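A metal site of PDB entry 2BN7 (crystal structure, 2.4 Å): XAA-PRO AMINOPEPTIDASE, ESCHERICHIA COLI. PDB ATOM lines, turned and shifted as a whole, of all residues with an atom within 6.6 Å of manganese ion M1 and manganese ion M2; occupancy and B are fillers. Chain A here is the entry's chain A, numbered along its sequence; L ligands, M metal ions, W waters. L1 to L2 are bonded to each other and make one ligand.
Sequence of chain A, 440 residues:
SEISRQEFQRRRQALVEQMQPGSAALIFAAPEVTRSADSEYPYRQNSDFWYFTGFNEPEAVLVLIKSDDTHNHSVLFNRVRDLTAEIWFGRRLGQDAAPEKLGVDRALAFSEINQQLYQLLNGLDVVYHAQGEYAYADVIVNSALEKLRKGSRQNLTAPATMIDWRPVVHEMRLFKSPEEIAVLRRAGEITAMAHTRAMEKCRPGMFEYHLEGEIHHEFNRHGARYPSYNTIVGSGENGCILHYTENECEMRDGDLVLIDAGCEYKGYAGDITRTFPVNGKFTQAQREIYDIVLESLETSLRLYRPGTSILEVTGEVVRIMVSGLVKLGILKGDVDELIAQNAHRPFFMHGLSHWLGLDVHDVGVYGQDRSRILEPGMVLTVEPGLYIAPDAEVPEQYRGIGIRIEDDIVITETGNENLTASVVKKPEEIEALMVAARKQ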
ATOM      1  N   TYR A 229      15.373  -4.816   2.653  1.00  0.00           N
ATOM      2  CA  TYR A 229      16.521  -5.494   3.238  1.00  0.00           C
ATOM      3  C   TYR A 229      16.038  -6.647   4.107  1.00  0.00           C
ATOM      4  O   TYR A 229      14.856  -6.724   4.449  1.00  0.00           O
ATOM      5  CB  TYR A 229      17.381  -4.524   4.073  1.00  0.00           C
ATOM      6  CG  TYR A 229      16.605  -3.736   5.103  1.00  0.00           C
ATOM      7  CD1 TYR A 229      15.884  -2.610   4.724  1.00  0.00           C
ATOM      8  CD2 TYR A 229      16.587  -4.111   6.437  1.00  0.00           C
ATOM      9  CE1 TYR A 229      15.165  -1.884   5.647  1.00  0.00           C
ATOM     10  CE2 TYR A 229      15.873  -3.398   7.370  1.00  0.00           C
ATOM     11  CZ  TYR A 229      15.164  -2.267   6.971  1.00  0.00           C
ATOM     12  OH  TYR A 229      14.457  -1.537   7.873  1.00  0.00           O
ATOM     13  N   ILE A 232      15.309  -7.731  10.564  1.00  0.00           N
ATOM     14  CA  ILE A 232      16.054  -7.935  11.789  1.00  0.00           C
ATOM     15  C   ILE A 232      15.076  -7.942  12.960  1.00  0.00           C
ATOM     16  O   ILE A 232      14.377  -6.965  13.184  1.00  0.00           O
ATOM     17  CB  ILE A 232      17.093  -6.784  12.008  1.00  0.00           C
ATOM     18  CG1 ILE A 232      18.204  -6.851  10.947  1.00  0.00           C
ATOM     19  CG2 ILE A 232      17.680  -6.796  13.426  1.00  0.00           C
ATOM     20  CD1 ILE A 232      18.741  -5.492  10.554  1.00  0.00           C
ATOM     21  N   ASP A 260      14.231  -4.046  13.107  1.00  0.00           N
ATOM     22  CA  ASP A 260      14.615  -3.197  11.988  1.00  0.00           C
ATOM     23  C   ASP A 260      14.088  -3.835  10.696  1.00  0.00           C
ATOM     24  O   ASP A 260      14.571  -4.887  10.264  1.00  0.00           O
ATOM     25  CB  ASP A 260      16.135  -3.022  11.940  1.00  0.00           C
ATOM     26  CG  ASP A 260      16.565  -1.822  11.119  1.00  0.00           C
ATOM     27  OD1 ASP A 260      15.783  -1.300  10.298  1.00  0.00           O
ATOM     28  OD2 ASP A 260      17.724  -1.400  11.298  1.00  0.00           O
ATOM     29  N   ALA A 261      13.077  -3.199  10.105  1.00  0.00           N
ATOM     30  CA  ALA A 261      12.429  -3.758   8.910  1.00  0.00           C
ATOM     31  C   ALA A 261      11.827  -2.659   8.030  1.00  0.00           C
ATOM     32  O   ALA A 261      11.351  -1.648   8.515  1.00  0.00           O
ATOM     33  CB  ALA A 261      11.350  -4.778   9.327  1.00  0.00           C
ATOM     34  N   ASP A 271      12.464   2.118   5.998  1.00  0.00           N
ATOM     35  CA  ASP A 271      13.508   1.671   6.914  1.00  0.00           C
ATOM     36  C   ASP A 271      13.206   2.157   8.328  1.00  0.00           C
ATOM     37  O   ASP A 271      13.579   3.274   8.710  1.00  0.00           O
ATOM     38  CB  ASP A 271      14.872   2.185   6.442  1.00  0.00           C
ATOM     39  CG  ASP A 271      16.008   1.659   7.267  1.00  0.00           C
ATOM     40  OD1 ASP A 271      15.743   0.875   8.201  1.00  0.00           O
ATOM     41  OD2 ASP A 271      17.157   2.045   6.992  1.00  0.00           O
ATOM     42  N   ILE A 272      12.526   1.311   9.093  1.00  0.00           N
ATOM     43  CA  ILE A 272      12.127   1.660  10.452  1.00  0.00           C
ATOM     44  C   ILE A 272      12.748   0.683  11.464  1.00  0.00           C
ATOM     45  O   ILE A 272      12.852  -0.526  11.206  1.00  0.00           O
ATOM     46  CB  ILE A 272      10.585   1.637  10.603  1.00  0.00           C
ATOM     47  CG1 ILE A 272       9.950   2.756   9.776  1.00  0.00           C
ATOM     48  CG2 ILE A 272      10.185   1.768  12.090  1.00  0.00           C
ATOM     49  CD1 ILE A 272       8.424   2.838   9.908  1.00  0.00           C
ATOM     50  N   THR A 273      13.162   1.233  12.605  1.00  0.00           N
ATOM     51  CA  THR A 273      13.510   0.417  13.758  1.00  0.00           C
ATOM     52  C   THR A 273      12.649   0.869  14.921  1.00  0.00           C
ATOM     53  O   THR A 273      12.500   2.067  15.173  1.00  0.00           O
ATOM     54  CB  THR A 273      15.009   0.483  14.177  1.00  0.00           C
ATOM     55  OG1 THR A 273      15.845   0.263  13.044  1.00  0.00           O
ATOM     56  CG2 THR A 273      15.308  -0.607  15.199  1.00  0.00           C
ATOM     57  N   HIS A 354      21.763   7.526   7.253  1.00  0.00           N
ATOM     58  CA  HIS A 354      22.221   7.240   5.905  1.00  0.00           C
ATOM     59  C   HIS A 354      21.183   7.725   4.906  1.00  0.00           C
ATOM     60  O   HIS A 354      20.012   7.893   5.253  1.00  0.00           O
ATOM     61  CB  HIS A 354      22.535   5.744   5.691  1.00  0.00           C
ATOM     62  CG  HIS A 354      21.396   4.824   5.994  1.00  0.00           C
ATOM     63  ND1 HIS A 354      20.327   4.640   5.135  1.00  0.00           N
ATOM     64  CD2 HIS A 354      21.176   3.996   7.040  1.00  0.00           C
ATOM     65  CE1 HIS A 354      19.492   3.761   5.656  1.00  0.00           C
ATOM     66  NE2 HIS A 354      19.983   3.350   6.819  1.00  0.00           N
ATOM     67  N   LEU A 356      18.508   7.530   1.909  1.00  0.00           N
ATOM     68  CA  LEU A 356      17.452   6.534   1.682  1.00  0.00           C
ATOM     69  C   LEU A 356      16.782   6.758   0.322  1.00  0.00           C
ATOM     70  O   LEU A 356      16.465   7.898  -0.051  1.00  0.00           O
ATOM     71  CB  LEU A 356      16.400   6.635   2.795  1.00  0.00           C
ATOM     72  CG  LEU A 356      15.291   5.577   2.794  1.00  0.00           C
ATOM     73  CD1 LEU A 356      15.843   4.189   3.128  1.00  0.00           C
ATOM     74  CD2 LEU A 356      14.205   5.973   3.786  1.00  0.00           C
ATOM     75  N   VAL A 360      18.260   0.985   0.327  1.00  0.00           N
ATOM     76  CA  VAL A 360      18.045   1.331   1.726  1.00  0.00           C
ATOM     77  C   VAL A 360      19.233   2.164   2.226  1.00  0.00           C
ATOM     78  O   VAL A 360      19.044   3.236   2.793  1.00  0.00           O
ATOM     79  CB  VAL A 360      17.704   0.067   2.600  1.00  0.00           C
ATOM     80  CG1 VAL A 360      18.846  -0.950   2.619  1.00  0.00           C
ATOM     81  CG2 VAL A 360      17.319   0.490   4.019  1.00  0.00           C
ATOM     82  N   HIS A 361      20.457   1.699   1.976  1.00  0.00           N
ATOM     83  CA  HIS A 361      21.645   2.534   2.128  1.00  0.00           C
ATOM     84  C   HIS A 361      21.923   3.167   0.770  1.00  0.00           C
ATOM     85  O   HIS A 361      22.617   2.582  -0.068  1.00  0.00           O
ATOM     86  CB  HIS A 361      22.850   1.710   2.572  1.00  0.00           C
ATOM     87  CG  HIS A 361      22.652   1.039   3.886  1.00  0.00           C
ATOM     88  ND1 HIS A 361      23.389  -0.062   4.274  1.00  0.00           N
ATOM     89  CD2 HIS A 361      21.785   1.280   4.890  1.00  0.00           C
ATOM     90  CE1 HIS A 361      22.994  -0.448   5.475  1.00  0.00           C
ATOM     91  NE2 HIS A 361      22.022   0.358   5.870  1.00  0.00           N
ATOM     92  N   THR A 381      17.792   8.531   7.009  1.00  0.00           N
ATOM     93  CA  THR A 381      17.323   7.906   8.221  1.00  0.00           C
ATOM     94  C   THR A 381      17.850   8.674   9.427  1.00  0.00           C
ATOM     95  O   THR A 381      18.776   9.471   9.308  1.00  0.00           O
ATOM     96  CB  THR A 381      17.782   6.453   8.315  1.00  0.00           C
ATOM     97  OG1 THR A 381      19.205   6.399   8.458  1.00  0.00           O
ATOM     98  CG2 THR A 381      17.325   5.696   7.062  1.00  0.00           C
ATOM     99  N   VAL A 382      17.204   8.448  10.564  1.00  0.00           N
ATOM    100  CA  VAL A 382      17.634   9.004  11.838  1.00  0.00           C
ATOM    101  C   VAL A 382      17.511   7.857  12.814  1.00  0.00           C
ATOM    102  O   VAL A 382      16.400   7.505  13.203  1.00  0.00           O
ATOM    103  CB  VAL A 382      16.767  10.221  12.289  1.00  0.00           C
ATOM    104  CG1 VAL A 382      17.397  10.930  13.489  1.00  0.00           C
ATOM    105  CG2 VAL A 382      16.585  11.208  11.152  1.00  0.00           C
ATOM    106  N   GLU A 383      18.632   7.274  13.193  1.00  0.00           N
ATOM    107  CA  GLU A 383      18.632   6.014  13.946  1.00  0.00           C
ATOM    108  C   GLU A 383      19.694   5.925  15.032  1.00  0.00           C
ATOM    109  O   GLU A 383      20.617   5.113  14.945  1.00  0.00           O
ATOM    110  CB  GLU A 383      18.774   4.840  12.973  1.00  0.00           C
ATOM    111  CG  GLU A 383      19.932   4.934  12.007  1.00  0.00           C
ATOM    112  CD  GLU A 383      19.961   3.777  11.054  1.00  0.00           C
ATOM    113  OE1 GLU A 383      19.880   2.613  11.540  1.00  0.00           O
ATOM    114  OE2 GLU A 383      20.059   4.025   9.840  1.00  0.00           O
ATOM    115  N   ARG A 404      17.549   0.449  19.367  1.00  0.00           N
ATOM    116  CA  ARG A 404      17.628   1.418  18.274  1.00  0.00           C
ATOM    117  C   ARG A 404      16.212   1.918  18.002  1.00  0.00           C
ATOM    118  O   ARG A 404      15.249   1.155  18.126  1.00  0.00           O
ATOM    119  CB  ARG A 404      18.233   0.798  17.018  1.00  0.00           C
ATOM    120  CG  ARG A 404      18.292   1.725  15.802  1.00  0.00           C
ATOM    121  CD  ARG A 404      19.294   1.249  14.747  1.00  0.00           C
ATOM    122  NE  ARG A 404      18.953  -0.041  14.115  1.00  0.00           N
ATOM    123  CZ  ARG A 404      19.502  -1.225  14.422  1.00  0.00           C
ATOM    124  NH1 ARG A 404      20.441  -1.354  15.353  1.00  0.00           N
ATOM    125  NH2 ARG A 404      19.111  -2.300  13.767  1.00  0.00           N
ATOM    126  N   GLU A 406      14.527   4.203  14.884  1.00  0.00           N
ATOM    127  CA  GLU A 406      14.839   4.752  13.571  1.00  0.00           C
ATOM    128  C   GLU A 406      13.614   5.255  12.818  1.00  0.00           C
ATOM    129  O   GLU A 406      12.656   4.502  12.589  1.00  0.00           O
ATOM    130  CB  GLU A 406      15.539   3.686  12.727  1.00  0.00           C
ATOM    131  CG  GLU A 406      15.683   4.033  11.248  1.00  0.00           C
ATOM    132  CD  GLU A 406      16.513   3.029  10.515  1.00  0.00           C
ATOM    133  OE1 GLU A 406      16.507   1.845  10.933  1.00  0.00           O
ATOM    134  OE2 GLU A 406      17.164   3.414   9.524  1.00  0.00           O
ATOM    135  N   ASP A 408      12.449   7.745   9.175  1.00  0.00           N
ATOM    136  CA  ASP A 408      12.858   8.181   7.835  1.00  0.00           C
ATOM    137  C   ASP A 408      12.329   9.585   7.591  1.00  0.00           C
ATOM    138  O   ASP A 408      11.156   9.855   7.811  1.00  0.00           O
ATOM    139  CB  ASP A 408      12.260   7.257   6.764  1.00  0.00           C
ATOM    140  CG  ASP A 408      12.625   5.816   6.975  1.00  0.00           C
ATOM    141  OD1 ASP A 408      13.682   5.547   7.595  1.00  0.00           O
ATOM    142  OD2 ASP A 408      11.843   4.960   6.511  1.00  0.00           O
HETATM  143  N1  LIG L   1      21.559  -0.153  10.126  1.00  0.00           N
HETATM  144  C1  LIG L   1      22.496   0.950  10.264  1.00  0.00           C
HETATM  145  C2  LIG L   1      23.617   0.971   9.215  1.00  0.00           C
HETATM  146  O1  LIG L   1      23.865  -0.036   8.538  1.00  0.00           O
HETATM  147  C3  LIG L   1      23.100   0.726  11.653  1.00  0.00           C
HETATM  148  C4  LIG L   1      22.112  -0.089  12.379  1.00  0.00           C
HETATM  149  C5  LIG L   1      21.467  -0.950  11.362  1.00  0.00           C
HETATM  150  N1  LG2 L   2      24.272   2.123   9.101  1.00  0.00           N
HETATM  151  C1  LG2 L   2      25.469   2.312   8.271  1.00  0.00           C
HETATM  152  C2  LG2 L   2      26.542   2.996   9.112  1.00  0.00           C
HETATM  153  O1  LG2 L   2      27.733   2.705   9.029  1.00  0.00           O
HETATM  154  C3  LG2 L   2      25.146   3.158   7.023  1.00  0.00           C
HETATM  155  C4  LG2 L   2      26.275   3.376   5.991  1.00  0.00           C
HETATM  156  C5  LG2 L   2      26.650   2.093   5.276  1.00  0.00           C
HETATM  157  C6  LG2 L   2      25.874   4.426   4.981  1.00  0.00           C
HETATM  158  O2  LG2 L   2      26.228   3.881   9.915  1.00  0.00           O
HETATM  159 MN    MN M   1      18.746   2.649   8.435  1.00  0.00          MN
HETATM  160 MN    MN M   2      17.128   0.255   9.656  1.00  0.00          MN
HETATM  161 ZN    ZN M   3      21.774  -1.147   7.837  1.00  0.00          ZN
HETATM  162  O   HOH W   1      19.181   0.995   9.459  1.00  0.00           O
HETATM  163  O   HOH W   2      18.873  -1.483   7.446  1.00  0.00           O
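OE1 of Glu 383 lies close to N1 of LIG L1, at 3.5 Å.
OG1 of Thr 273 lies within hydrogen-bond range of NE of Arg 404 (3.3 Å).
The backbone NH of Glu 406 is in hydrogen-bond range of the backbone carbonyl oxygen of Thr 273, at 3.0 Å.
The backbone carbonyl oxygen of Ile 232 lies within hydrogen-bond range of the backbone NH of Asp 260.
OE2 of Glu 383 sits close to OG1 of Thr 381.
The side-chain carboxylate of Glu 383 lies within salt-bridge range of the guanidinium group of Arg 404 (3.8 Å).
The side-chain carboxylate (OD2) of Asp 260 sits close to the side-chain hydroxyl (OG1) of Thr 273.
The side-chain carboxylate of Asp 260 sits close to the side-chain hydroxyl of Tyr 229 (2.8 Å).
OD1 of Asp 271 lies close to OH of Tyr 229 (2.8 Å).
CG2 of Thr 381 touches manganese ion M1, 3.6 Å away.
Of the 17 residues printed, 5 come within 4 Å of manganese ion M1.
Along chain A the residues within 4 Å of manganese ion M1 span positions 271 to 406.
Merely in contact with manganese ion M2: Thr 273 (3.6 Å) and Tyr 229 (3.7 Å).
Five residues have an atom within 4 Å of manganese ion M2: Tyr 229, Asp 260, Asp 271, Thr 273 and Glu 406.
Manganese ion M1 is bound by water W1 (2.0 Å), the side-chain carboxylate (OE2) of Glu 406 (2.1 Å), a ring nitrogen (NE2) of His 354 (2.2 Å), the side-chain carboxylate (OD2) of Asp 271 (2.2 Å) and the side-chain carboxylate (OE2) of Glu 383 (2.4 Å).
Manganese ion M1 has five donor atoms within binding distance.
Manganese ion M2 is bound by the side-chain carboxylate (OD1) of Asp 271, at 2.1 Å.
The side-chain carboxylate (OE1) of Glu 406 binds manganese ion M2 (2.1 Å).
The side-chain carboxylate (OD1) of Asp 260 binds manganese ion M2, 2.2 Å away.
Water W1 binds manganese ion M2 (2.2 Å).
Manganese ion M2 is bound by OD2 of Asp 260.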
